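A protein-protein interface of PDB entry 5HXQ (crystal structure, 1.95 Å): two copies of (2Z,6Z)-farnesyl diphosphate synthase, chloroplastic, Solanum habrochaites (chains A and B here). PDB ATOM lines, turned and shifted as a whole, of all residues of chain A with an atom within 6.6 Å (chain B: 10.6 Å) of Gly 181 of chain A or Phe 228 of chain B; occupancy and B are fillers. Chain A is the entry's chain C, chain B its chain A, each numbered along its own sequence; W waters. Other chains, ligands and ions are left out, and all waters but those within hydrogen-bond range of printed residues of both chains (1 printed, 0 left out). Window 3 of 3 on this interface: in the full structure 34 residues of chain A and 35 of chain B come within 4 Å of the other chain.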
ATOM      1  N   ILE A  14     -16.624 -13.893 -19.445  1.00  0.00           N
ATOM      2  CA  ILE A  14     -17.954 -13.551 -19.950  1.00  0.00           C
ATOM      3  C   ILE A  14     -18.917 -14.638 -19.469  1.00  0.00           C
ATOM      4  O   ILE A  14     -18.908 -15.744 -19.976  1.00  0.00           O
ATOM      5  CB  ILE A  14     -17.990 -13.395 -21.473  1.00  0.00           C
ATOM      6  CG1 ILE A  14     -17.030 -12.272 -21.903  1.00  0.00           C
ATOM      7  CG2 ILE A  14     -19.417 -13.088 -21.940  1.00  0.00           C
ATOM      8  CD1 ILE A  14     -16.958 -12.014 -23.392  1.00  0.00           C
ATOM      9  N   MET A  15     -19.748 -14.281 -18.495  1.00  0.00           N
ATOM     10  CA  MET A  15     -20.507 -15.244 -17.685  1.00  0.00           C
ATOM     11  C   MET A  15     -21.879 -15.512 -18.301  1.00  0.00           C
ATOM     12  O   MET A  15     -22.900 -15.121 -17.727  1.00  0.00           O
ATOM     13  CB  MET A  15     -20.688 -14.678 -16.269  1.00  0.00           C
ATOM     14  CG  MET A  15     -19.403 -14.200 -15.615  1.00  0.00           C
ATOM     15  SD  MET A  15     -19.653 -13.636 -13.925  1.00  0.00           S
ATOM     16  CE  MET A  15     -20.473 -12.070 -14.201  1.00  0.00           C
ATOM     17  N   ASP A  16     -21.902 -16.161 -19.465  1.00  0.00           N
ATOM     18  CA  ASP A  16     -23.135 -16.325 -20.238  1.00  0.00           C
ATOM     19  C   ASP A  16     -23.712 -17.748 -20.096  1.00  0.00           C
ATOM     20  O   ASP A  16     -22.994 -18.704 -19.764  1.00  0.00           O
ATOM     21  CB  ASP A  16     -22.867 -15.989 -21.709  1.00  0.00           C
ATOM     22  CG  ASP A  16     -24.138 -15.963 -22.575  1.00  0.00           C
ATOM     23  OD1 ASP A  16     -25.262 -15.780 -22.035  1.00  0.00           O
ATOM     24  OD2 ASP A  16     -23.999 -16.109 -23.819  1.00  0.00           O
ATOM     25  N   GLY A  17     -25.009 -17.870 -20.356  1.00  0.00           N
ATOM     26  CA  GLY A  17     -25.692 -19.172 -20.323  1.00  0.00           C
ATOM     27  C   GLY A  17     -26.589 -19.384 -19.113  1.00  0.00           C
ATOM     28  O   GLY A  17     -27.095 -20.485 -18.897  1.00  0.00           O
ATOM     29  N   ARG A  20     -30.407 -19.728 -20.402  1.00  0.00           N
ATOM     30  CA  ARG A  20     -30.637 -21.005 -21.084  1.00  0.00           C
ATOM     31  C   ARG A  20     -30.563 -22.177 -20.113  1.00  0.00           C
ATOM     32  O   ARG A  20     -31.226 -23.194 -20.308  1.00  0.00           O
ATOM     33  CB  ARG A  20     -29.638 -21.228 -22.229  1.00  0.00           C
ATOM     34  CG  ARG A  20     -30.251 -21.960 -23.415  1.00  0.00           C
ATOM     35  CD  ARG A  20     -29.265 -22.839 -24.174  1.00  0.00           C
ATOM     36  NE  ARG A  20     -29.325 -24.245 -23.752  1.00  0.00           N
ATOM     37  CZ  ARG A  20     -28.900 -25.284 -24.478  1.00  0.00           C
ATOM     38  NH1 ARG A  20     -29.003 -26.516 -23.987  1.00  0.00           N
ATOM     39  NH2 ARG A  20     -28.375 -25.107 -25.692  1.00  0.00           N
ATOM     40  N   ARG A 179     -15.238 -17.487 -22.061  1.00  0.00           N
ATOM     41  CA  ARG A 179     -16.632 -17.213 -22.270  1.00  0.00           C
ATOM     42  C   ARG A 179     -17.419 -18.523 -22.252  1.00  0.00           C
ATOM     43  O   ARG A 179     -17.196 -19.413 -23.086  1.00  0.00           O
ATOM     44  CB  ARG A 179     -16.873 -16.495 -23.579  1.00  0.00           C
ATOM     45  CG  ARG A 179     -18.360 -16.336 -23.818  1.00  0.00           C
ATOM     46  CD  ARG A 179     -18.672 -15.361 -24.913  1.00  0.00           C
ATOM     47  NE  ARG A 179     -20.115 -15.202 -25.025  1.00  0.00           N
ATOM     48  CZ  ARG A 179     -20.722 -14.117 -25.484  1.00  0.00           C
ATOM     49  NH1 ARG A 179     -20.019 -13.066 -25.886  1.00  0.00           N
ATOM     50  NH2 ARG A 179     -22.043 -14.080 -25.538  1.00  0.00           N
ATOM     51  N   THR A 180     -18.330 -18.614 -21.289  1.00  0.00           N
ATOM     52  CA  THR A 180     -19.236 -19.757 -21.144  1.00  0.00           C
ATOM     53  C   THR A 180     -20.455 -19.529 -22.017  1.00  0.00           C
ATOM     54  O   THR A 180     -20.757 -18.398 -22.372  1.00  0.00           O
ATOM     55  CB  THR A 180     -19.688 -19.904 -19.677  1.00  0.00           C
ATOM     56  OG1 THR A 180     -20.275 -18.675 -19.210  1.00  0.00           O
ATOM     57  CG2 THR A 180     -18.522 -20.247 -18.798  1.00  0.00           C
ATOM     58  N   GLY A 181     -21.172 -20.593 -22.364  1.00  0.00           N
ATOM     59  CA  GLY A 181     -22.469 -20.427 -23.024  1.00  0.00           C
ATOM     60  C   GLY A 181     -22.506 -20.679 -24.510  1.00  0.00           C
ATOM     61  O   GLY A 181     -23.583 -20.690 -25.102  1.00  0.00           O
ATOM     62  N   GLY A 182     -21.340 -20.824 -25.136  1.00  0.00           N
ATOM     63  CA  GLY A 182     -21.264 -21.290 -26.516  1.00  0.00           C
ATOM     64  C   GLY A 182     -21.149 -20.254 -27.618  1.00  0.00           C
ATOM     65  O   GLY A 182     -20.824 -20.615 -28.752  1.00  0.00           O
ATOM     66  N   ASP A 183     -21.428 -18.982 -27.326  1.00  0.00           N
ATOM     67  CA  ASP A 183     -21.232 -17.954 -28.323  1.00  0.00           C
ATOM     68  C   ASP A 183     -19.733 -17.608 -28.404  1.00  0.00           C
ATOM     69  O   ASP A 183     -19.006 -17.662 -27.409  1.00  0.00           O
ATOM     70  CB  ASP A 183     -22.082 -16.706 -28.057  1.00  0.00           C
ATOM     71  CG  ASP A 183     -22.455 -15.963 -29.341  1.00  0.00           C
ATOM     72  OD1 ASP A 183     -22.190 -16.497 -30.428  1.00  0.00           O
ATOM     73  OD2 ASP A 183     -23.026 -14.850 -29.277  1.00  0.00           O
ATOM     74  N   GLN A 184     -19.279 -17.288 -29.604  1.00  0.00           N
ATOM     75  CA  GLN A 184     -17.862 -17.004 -29.833  1.00  0.00           C
ATOM     76  C   GLN A 184     -17.667 -15.546 -30.235  1.00  0.00           C
ATOM     77  O   GLN A 184     -17.103 -15.254 -31.268  1.00  0.00           O
ATOM     78  CB  GLN A 184     -17.278 -17.961 -30.876  1.00  0.00           C
ATOM     79  CG  GLN A 184     -17.341 -19.420 -30.449  1.00  0.00           C
ATOM     80  CD  GLN A 184     -16.231 -20.293 -31.015  1.00  0.00           C
ATOM     81  OE1 GLN A 184     -15.910 -21.332 -30.439  1.00  0.00           O
ATOM     82  NE2 GLN A 184     -15.644 -19.890 -32.147  1.00  0.00           N
ATOM     83  N   ARG A 185     -18.165 -14.642 -29.401  1.00  0.00           N
ATOM     84  CA  ARG A 185     -17.917 -13.223 -29.567  1.00  0.00           C
ATOM     85  C   ARG A 185     -17.530 -12.603 -28.228  1.00  0.00           C
ATOM     86  O   ARG A 185     -17.598 -13.260 -27.178  1.00  0.00           O
ATOM     87  CB  ARG A 185     -19.108 -12.502 -30.222  1.00  0.00           C
ATOM     88  CG  ARG A 185     -20.493 -13.051 -29.912  1.00  0.00           C
ATOM     89  CD  ARG A 185     -21.586 -12.004 -30.104  1.00  0.00           C
ATOM     90  NE  ARG A 185     -21.984 -11.828 -31.503  1.00  0.00           N
ATOM     91  CZ  ARG A 185     -22.998 -12.459 -32.106  1.00  0.00           C
ATOM     92  NH1 ARG A 185     -23.739 -13.356 -31.457  1.00  0.00           N
ATOM     93  NH2 ARG A 185     -23.266 -12.202 -33.384  1.00  0.00           N
ATOM     94  N   THR A 202     -16.319 -22.041 -24.375  1.00  0.00           N
ATOM     95  CA  THR A 202     -16.908 -23.333 -24.009  1.00  0.00           C
ATOM     96  C   THR A 202     -18.436 -23.295 -24.084  1.00  0.00           C
ATOM     97  O   THR A 202     -19.061 -22.279 -23.800  1.00  0.00           O
ATOM     98  CB  THR A 202     -16.455 -23.791 -22.612  1.00  0.00           C
ATOM     99  OG1 THR A 202     -17.068 -25.052 -22.297  1.00  0.00           O
ATOM    100  CG2 THR A 202     -16.815 -22.748 -21.538  1.00  0.00           C
ATOM    101  N   LYS A 203     -19.032 -24.410 -24.498  1.00  0.00           N
ATOM    102  CA  LYS A 203     -20.491 -24.564 -24.478  1.00  0.00           C
ATOM    103  C   LYS A 203     -21.060 -24.717 -23.064  1.00  0.00           C
ATOM    104  O   LYS A 203     -22.247 -24.527 -22.869  1.00  0.00           O
ATOM    105  CB  LYS A 203     -20.915 -25.763 -25.335  1.00  0.00           C
ATOM    106  CG  LYS A 203     -20.858 -25.474 -26.822  1.00  0.00           C
ATOM    107  CD  LYS A 203     -20.913 -26.750 -27.653  1.00  0.00           C
ATOM    108  CE  LYS A 203     -21.002 -26.423 -29.137  1.00  0.00           C
ATOM    109  NZ  LYS A 203     -21.159 -27.650 -29.974  1.00  0.00           N
ATOM    110  N   THR A 204     -20.222 -25.057 -22.088  1.00  0.00           N
ATOM    111  CA  THR A 204     -20.658 -25.139 -20.694  1.00  0.00           C
ATOM    112  C   THR A 204     -21.324 -23.843 -20.262  1.00  0.00           C
ATOM    113  O   THR A 204     -20.767 -22.753 -20.444  1.00  0.00           O
ATOM    114  CB  THR A 204     -19.494 -25.388 -19.728  1.00  0.00           C
ATOM    115  OG1 THR A 204     -18.761 -26.532 -20.149  1.00  0.00           O
ATOM    116  CG2 THR A 204     -19.995 -25.613 -18.311  1.00  0.00           C
ATOM    117  N   LEU A 205     -22.512 -23.980 -19.685  1.00  0.00           N
ATOM    118  CA  LEU A 205     -23.280 -22.849 -19.214  1.00  0.00           C
ATOM    119  C   LEU A 205     -22.674 -22.399 -17.895  1.00  0.00           C
ATOM    120  O   LEU A 205     -22.069 -23.194 -17.186  1.00  0.00           O
ATOM    121  CB  LEU A 205     -24.760 -23.234 -19.069  1.00  0.00           C
ATOM    122  CG  LEU A 205     -25.415 -23.855 -20.313  1.00  0.00           C
ATOM    123  CD1 LEU A 205     -26.836 -24.308 -19.992  1.00  0.00           C
ATOM    124  CD2 LEU A 205     -25.434 -22.907 -21.505  1.00  0.00           C
ATOM    125  N   PHE A 206     -22.793 -21.114 -17.588  1.00  0.00           N
ATOM    126  CA  PHE A 206     -22.068 -20.539 -16.456  1.00  0.00           C
ATOM    127  C   PHE A 206     -22.347 -21.249 -15.122  1.00  0.00           C
ATOM    128  O   PHE A 206     -21.412 -21.546 -14.370  1.00  0.00           O
ATOM    129  CB  PHE A 206     -22.325 -19.026 -16.338  1.00  0.00           C
ATOM    130  CG  PHE A 206     -21.435 -18.353 -15.333  1.00  0.00           C
ATOM    131  CD1 PHE A 206     -20.059 -18.318 -15.531  1.00  0.00           C
ATOM    132  CD2 PHE A 206     -21.961 -17.776 -14.181  1.00  0.00           C
ATOM    133  CE1 PHE A 206     -19.224 -17.728 -14.599  1.00  0.00           C
ATOM    134  CE2 PHE A 206     -21.130 -17.179 -13.250  1.00  0.00           C
ATOM    135  CZ  PHE A 206     -19.762 -17.154 -13.458  1.00  0.00           C
ATOM    136  N   LEU B   6     -28.400 -16.489 -45.304  1.00  0.00           N
ATOM    137  CA  LEU B   6     -27.640 -16.109 -44.077  1.00  0.00           C
ATOM    138  C   LEU B   6     -26.129 -16.049 -44.379  1.00  0.00           C
ATOM    139  O   LEU B   6     -25.327 -16.773 -43.792  1.00  0.00           O
ATOM    140  CB  LEU B   6     -27.958 -17.097 -42.940  1.00  0.00           C
ATOM    141  CG  LEU B   6     -27.888 -16.611 -41.481  1.00  0.00           C
ATOM    142  CD1 LEU B   6     -28.104 -17.783 -40.529  1.00  0.00           C
ATOM    143  CD2 LEU B   6     -26.584 -15.895 -41.143  1.00  0.00           C
ATOM    144  N   ASP B 175     -18.859  -9.418 -39.726  1.00  0.00           N
ATOM    145  CA  ASP B 175     -19.806 -10.362 -39.162  1.00  0.00           C
ATOM    146  C   ASP B 175     -19.065 -11.587 -38.641  1.00  0.00           C
ATOM    147  O   ASP B 175     -19.450 -12.175 -37.639  1.00  0.00           O
ATOM    148  CB  ASP B 175     -20.768 -10.827 -40.248  1.00  0.00           C
ATOM    149  CG  ASP B 175     -21.550  -9.705 -40.814  1.00  0.00           C
ATOM    150  OD1 ASP B 175     -22.398  -9.194 -40.059  1.00  0.00           O
ATOM    151  OD2 ASP B 175     -21.309  -9.309 -41.982  1.00  0.00           O
ATOM    152  N   TYR B 196     -18.868  -7.166 -31.926  1.00  0.00           N
ATOM    153  CA  TYR B 196     -19.914  -8.212 -32.036  1.00  0.00           C
ATOM    154  C   TYR B 196     -19.656  -9.294 -33.084  1.00  0.00           C
ATOM    155  O   TYR B 196     -20.501 -10.180 -33.294  1.00  0.00           O
ATOM    156  CB  TYR B 196     -21.271  -7.556 -32.313  1.00  0.00           C
ATOM    157  CG  TYR B 196     -21.710  -6.723 -31.161  1.00  0.00           C
ATOM    158  CD1 TYR B 196     -22.278  -7.311 -30.049  1.00  0.00           C
ATOM    159  CD2 TYR B 196     -21.560  -5.342 -31.178  1.00  0.00           C
ATOM    160  CE1 TYR B 196     -22.694  -6.547 -28.979  1.00  0.00           C
ATOM    161  CE2 TYR B 196     -21.981  -4.570 -30.111  1.00  0.00           C
ATOM    162  CZ  TYR B 196     -22.537  -5.181 -29.017  1.00  0.00           C
ATOM    163  OH  TYR B 196     -22.929  -4.427 -27.941  1.00  0.00           O
ATOM    164  N   THR B 197     -18.489  -9.229 -33.715  1.00  0.00           N
ATOM    165  CA  THR B 197     -18.060 -10.201 -34.698  1.00  0.00           C
ATOM    166  C   THR B 197     -17.960 -11.605 -34.120  1.00  0.00           C
ATOM    167  O   THR B 197     -17.410 -11.794 -33.053  1.00  0.00           O
ATOM    168  CB  THR B 197     -16.652  -9.838 -35.216  1.00  0.00           C
ATOM    169  OG1 THR B 197     -16.647  -8.482 -35.659  1.00  0.00           O
ATOM    170  CG2 THR B 197     -16.239 -10.741 -36.356  1.00  0.00           C
ATOM    171  N   GLU B 198     -18.452 -12.597 -34.852  1.00  0.00           N
ATOM    172  CA  GLU B 198     -18.270 -13.983 -34.446  1.00  0.00           C
ATOM    173  C   GLU B 198     -16.873 -14.446 -34.826  1.00  0.00           C
ATOM    174  O   GLU B 198     -16.423 -14.216 -35.950  1.00  0.00           O
ATOM    175  CB  GLU B 198     -19.298 -14.897 -35.129  1.00  0.00           C
ATOM    176  CG  GLU B 198     -20.719 -14.754 -34.615  1.00  0.00           C
ATOM    177  CD  GLU B 198     -20.922 -15.368 -33.248  1.00  0.00           C
ATOM    178  OE1 GLU B 198     -20.120 -16.246 -32.849  1.00  0.00           O
ATOM    179  OE2 GLU B 198     -21.902 -14.975 -32.575  1.00  0.00           O
ATOM    180  N   PHE B 199     -16.205 -15.138 -33.912  1.00  0.00           N
ATOM    181  CA  PHE B 199     -14.848 -15.621 -34.169  1.00  0.00           C
ATOM    182  C   PHE B 199     -14.821 -17.083 -34.588  1.00  0.00           C
ATOM    183  O   PHE B 199     -15.544 -17.934 -34.037  1.00  0.00           O
ATOM    184  CB  PHE B 199     -13.979 -15.411 -32.937  1.00  0.00           C
ATOM    185  CG  PHE B 199     -13.597 -13.979 -32.709  1.00  0.00           C
ATOM    186  CD1 PHE B 199     -12.480 -13.445 -33.326  1.00  0.00           C
ATOM    187  CD2 PHE B 199     -14.351 -13.162 -31.895  1.00  0.00           C
ATOM    188  CE1 PHE B 199     -12.129 -12.124 -33.122  1.00  0.00           C
ATOM    189  CE2 PHE B 199     -13.999 -11.834 -31.683  1.00  0.00           C
ATOM    190  CZ  PHE B 199     -12.897 -11.315 -32.297  1.00  0.00           C
ATOM    191  N   ASN B 220     -20.517 -22.779 -39.791  1.00  0.00           N
ATOM    192  CA  ASN B 220     -20.358 -22.579 -38.351  1.00  0.00           C
ATOM    193  C   ASN B 220     -20.906 -21.234 -37.889  1.00  0.00           C
ATOM    194  O   ASN B 220     -21.521 -21.141 -36.830  1.00  0.00           O
ATOM    195  CB  ASN B 220     -18.881 -22.727 -37.962  1.00  0.00           C
ATOM    196  CG  ASN B 220     -18.655 -22.614 -36.468  1.00  0.00           C
ATOM    197  OD1 ASN B 220     -18.679 -21.518 -35.909  1.00  0.00           O
ATOM    198  ND2 ASN B 220     -18.423 -23.748 -35.814  1.00  0.00           N
ATOM    199  N   PHE B 221     -20.678 -20.195 -38.686  1.00  0.00           N
ATOM    200  CA  PHE B 221     -21.252 -18.873 -38.422  1.00  0.00           C
ATOM    201  C   PHE B 221     -22.795 -18.887 -38.460  1.00  0.00           C
ATOM    202  O   PHE B 221     -23.458 -18.291 -37.603  1.00  0.00           O
ATOM    203  CB  PHE B 221     -20.693 -17.851 -39.426  1.00  0.00           C
ATOM    204  CG  PHE B 221     -21.435 -16.551 -39.451  1.00  0.00           C
ATOM    205  CD1 PHE B 221     -21.255 -15.617 -38.442  1.00  0.00           C
ATOM    206  CD2 PHE B 221     -22.316 -16.258 -40.489  1.00  0.00           C
ATOM    207  CE1 PHE B 221     -21.939 -14.419 -38.458  1.00  0.00           C
ATOM    208  CE2 PHE B 221     -23.003 -15.054 -40.513  1.00  0.00           C
ATOM    209  CZ  PHE B 221     -22.813 -14.133 -39.499  1.00  0.00           C
ATOM    210  N   GLN B 222     -23.351 -19.564 -39.461  1.00  0.00           N
ATOM    211  CA  GLN B 222     -24.797 -19.635 -39.640  1.00  0.00           C
ATOM    212  C   GLN B 222     -25.470 -20.316 -38.445  1.00  0.00           C
ATOM    213  O   GLN B 222     -26.437 -19.785 -37.902  1.00  0.00           O
ATOM    214  CB  GLN B 222     -25.133 -20.332 -40.965  1.00  0.00           C
ATOM    215  CG  GLN B 222     -24.781 -19.457 -42.169  1.00  0.00           C
ATOM    216  CD  GLN B 222     -24.743 -20.184 -43.506  1.00  0.00           C
ATOM    217  OE1 GLN B 222     -24.665 -21.405 -43.574  1.00  0.00           O
ATOM    218  NE2 GLN B 222     -24.769 -19.414 -44.584  1.00  0.00           N
ATOM    219  N   GLN B 223     -24.926 -21.454 -38.014  1.00  0.00           N
ATOM    220  CA  GLN B 223     -25.416 -22.158 -36.819  1.00  0.00           C
ATOM    221  C   GLN B 223     -25.370 -21.283 -35.581  1.00  0.00           C
ATOM    222  O   GLN B 223     -26.285 -21.282 -34.764  1.00  0.00           O
ATOM    223  CB  GLN B 223     -24.558 -23.379 -36.526  1.00  0.00           C
ATOM    224  CG  GLN B 223     -24.721 -24.530 -37.488  1.00  0.00           C
ATOM    225  CD  GLN B 223     -23.821 -25.692 -37.123  1.00  0.00           C
ATOM    226  OE1 GLN B 223     -22.784 -25.511 -36.480  1.00  0.00           O
ATOM    227  NE2 GLN B 223     -24.215 -26.896 -37.524  1.00  0.00           N
ATOM    228  N   ARG B 224     -24.276 -20.548 -35.439  1.00  0.00           N
ATOM    229  CA  ARG B 224     -24.080 -19.694 -34.281  1.00  0.00           C
ATOM    230  C   ARG B 224     -25.011 -18.494 -34.338  1.00  0.00           C
ATOM    231  O   ARG B 224     -25.513 -18.045 -33.308  1.00  0.00           O
ATOM    232  CB  ARG B 224     -22.620 -19.247 -34.201  1.00  0.00           C
ATOM    233  CG  ARG B 224     -22.163 -18.866 -32.806  1.00  0.00           C
ATOM    234  CD  ARG B 224     -20.701 -19.227 -32.621  1.00  0.00           C
ATOM    235  NE  ARG B 224     -20.521 -20.661 -32.406  1.00  0.00           N
ATOM    236  CZ  ARG B 224     -19.422 -21.348 -32.718  1.00  0.00           C
ATOM    237  NH1 ARG B 224     -19.374 -22.651 -32.477  1.00  0.00           N
ATOM    238  NH2 ARG B 224     -18.371 -20.751 -33.276  1.00  0.00           N
ATOM    239  N   HIS B 225     -25.242 -17.986 -35.546  1.00  0.00           N
ATOM    240  CA  HIS B 225     -26.177 -16.885 -35.760  1.00  0.00           C
ATOM    241  C   HIS B 225     -27.624 -17.295 -35.435  1.00  0.00           C
ATOM    242  O   HIS B 225     -28.390 -16.497 -34.885  1.00  0.00           O
ATOM    243  CB  HIS B 225     -26.080 -16.398 -37.205  1.00  0.00           C
ATOM    244  CG  HIS B 225     -26.838 -15.136 -37.471  1.00  0.00           C
ATOM    245  ND1 HIS B 225     -28.155 -15.130 -37.876  1.00  0.00           N
ATOM    246  CD2 HIS B 225     -26.459 -13.838 -37.400  1.00  0.00           C
ATOM    247  CE1 HIS B 225     -28.558 -13.883 -38.035  1.00  0.00           C
ATOM    248  NE2 HIS B 225     -27.549 -13.079 -37.754  1.00  0.00           N
ATOM    249  N   ARG B 226     -27.984 -18.535 -35.775  1.00  0.00           N
ATOM    250  CA  ARG B 226     -29.300 -19.096 -35.431  1.00  0.00           C
ATOM    251  C   ARG B 226     -29.466 -19.240 -33.920  1.00  0.00           C
ATOM    252  O   ARG B 226     -30.503 -18.868 -33.367  1.00  0.00           O
ATOM    253  CB  ARG B 226     -29.498 -20.464 -36.087  1.00  0.00           C
ATOM    254  CG  ARG B 226     -29.604 -20.433 -37.604  1.00  0.00           C
ATOM    255  CD  ARG B 226     -29.422 -21.826 -38.186  1.00  0.00           C
ATOM    256  NE  ARG B 226     -28.863 -21.805 -39.537  1.00  0.00           N
ATOM    257  CZ  ARG B 226     -28.394 -22.875 -40.178  1.00  0.00           C
ATOM    258  NH1 ARG B 226     -28.407 -24.074 -39.602  1.00  0.00           N
ATOM    259  NH2 ARG B 226     -27.905 -22.747 -41.408  1.00  0.00           N
ATOM    260  N   ARG B 227     -28.445 -19.796 -33.269  1.00  0.00           N
ATOM    261  CA  ARG B 227     -28.383 -19.873 -31.805  1.00  0.00           C
ATOM    262  C   ARG B 227     -28.368 -18.484 -31.157  1.00  0.00           C
ATOM    263  O   ARG B 227     -29.157 -18.211 -30.252  1.00  0.00           O
ATOM    264  CB  ARG B 227     -27.134 -20.651 -31.358  1.00  0.00           C
ATOM    265  CG  ARG B 227     -27.302 -22.164 -31.300  1.00  0.00           C
ATOM    266  CD  ARG B 227     -27.689 -22.631 -29.898  1.00  0.00           C
ATOM    267  NE  ARG B 227     -28.381 -23.924 -29.899  1.00  0.00           N
ATOM    268  CZ  ARG B 227     -27.795 -25.113 -30.049  1.00  0.00           C
ATOM    269  NH1 ARG B 227     -26.478 -25.217 -30.229  1.00  0.00           N
ATOM    270  NH2 ARG B 227     -28.539 -26.217 -30.027  1.00  0.00           N
ATOM    271  N   PHE B 228     -27.467 -17.620 -31.632  1.00  0.00           N
ATOM    272  CA  PHE B 228     -27.273 -16.272 -31.080  1.00  0.00           C
ATOM    273  C   PHE B 228     -27.305 -15.230 -32.203  1.00  0.00           C
ATOM    274  O   PHE B 228     -28.351 -14.670 -32.533  1.00  0.00           O
ATOM    275  CB  PHE B 228     -25.923 -16.173 -30.340  1.00  0.00           C
ATOM    276  CG  PHE B 228     -25.555 -17.410 -29.555  1.00  0.00           C
ATOM    277  CD1 PHE B 228     -25.950 -17.557 -28.231  1.00  0.00           C
ATOM    278  CD2 PHE B 228     -24.804 -18.429 -30.140  1.00  0.00           C
ATOM    279  CE1 PHE B 228     -25.610 -18.694 -27.513  1.00  0.00           C
ATOM    280  CE2 PHE B 228     -24.468 -19.569 -29.424  1.00  0.00           C
ATOM    281  CZ  PHE B 228     -24.872 -19.699 -28.110  1.00  0.00           C
HETATM  282  O   HOH W   1     -21.766 -11.690 -36.063  1.00  0.00           O
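O of Tyr 196 of chain B is in hydrogen-bond range of NE of Arg 185 of chain A, 2.9 Å away. The side-chain carboxylate of Glu 198 of chain B lies close to the side-chain carboxylate of Asp 183 of chain A (2.6 Å). OE2 of Glu 198 of chain B lies within salt-bridge range of NH1 of Arg 185 of chain A (2.7 Å). NE2 of Gln 184 of chain A is in hydrogen-bond range of O of Phe 199 of chain B. NH2 of Arg 224 of chain B sits close to NE2 of Gln 184 of chain A.
N of Glu 198 of chain B sits at hydrogen-bond distance from O of Asp 175 of chain B (3.0 Å). NH2 of Arg 179 of chain A lies within salt-bridge range of OD2 of Asp 183 of chain A (3.9 Å). The backbone carbonyl oxygen of Arg 185 of chain A lies within hydrogen-bond range of the guanidinium group of Arg 179 of chain A (2.8 Å). O of Thr 204 of chain A sits at hydrogen-bond distance from N of Gly 181 of chain A, at 2.9 Å. The backbone carbonyl oxygen (O) of Thr 202 of chain A is in hydrogen-bond range of the backbone NH (N) of Gly 182 of chain A (3.0 Å). OD2 of Asp 183 of chain A is in salt-bridge range of NH1 of Arg 185 of chain A (2.7 Å).
Among the printed residues, merely in contact across the chains: Gly 181 of chain A with Phe 228 of chain B (3.4 Å), Gly 182 of chain A with Arg 224 of chain B (3.7 Å), Gly 182 of chain A with Phe 228 of chain B (3.8 Å), Asp 183 of chain A with Arg 224 of chain B (3.4 Å), Asp 183 of chain A with Phe 228 of chain B (3.3 Å), Gln 184 of chain A with Thr 197 of chain B (3.9 Å), Gln 184 of chain A with Glu 198 of chain B (3.5 Å), Arg 185 of chain A with Thr 197 of chain B (3.4 Å) and Arg 185 of chain A with Phe 228 of chain B (3.7 Å).
Gly 181 of chain A touches just one residue of chain B: Phe 228 (3.4 Å). Phe 228 of chain B touches just these residues of chain A: Gly 181 (3.4 Å), Gly 182 (3.8 Å), Asp 183 (3.3 Å) and Arg 185 (3.7 Å). No residue of chain B comes within 4 Å of Gly 17 of chain A. Thr 180 of chain A touches none of the printed residues of chain B. No residue of chain B comes within 4 Å of Thr 202 of chain A. Of the printed residues of chain B, Arg 185 of chain A touches Tyr 196, Thr 197, Glu 198 and Phe 228. Of the printed residues of chain B, Gln 184 of chain A touches Thr 197, Glu 198, Phe 199 and Arg 224. Of the printed residues of chain A, Tyr 196 of chain B touches Arg 185. Printed residues of chain A within 4 Å of Phe 199 of chain B: Gln 184. Ile 14 of chain A touches none of the printed residues of chain B. The nearest residue of chain A that does not touch Phe 228 of chain B is Asp 16 of chain A (4.8 Å).
Of the 17 printed residues of chain A, 5 touch a printed residue of chain B. Of the 15 printed residues of chain B, 6 touch a printed residue of chain A. Hydrophobic or aromatic side chains of chain B that line the printed part of chain A: Phe 199 and Phe 228. Along chain B the printed residues that touch a printed residue of chain A span positions 196 to 228. Among the printed residues, Asp or Glu carboxylates within 4 Å of a Lys or Arg side-chain nitrogen of the other chain: Arg 185 of chain A with Glu 198 of chain B (2.7 Å).
No position is printed for both chains. Of the 14 pairs that touch across the chains among the printed residues, none has its exchanged pair printed and touching as well.
Water W1 lies within hydrogen-bond range of O of Asp 175 of chain B (2.8 Å), NH2 of Arg 185 of chain A (3.1 Å) and O of Tyr 196 of chain B (3.4 Å).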
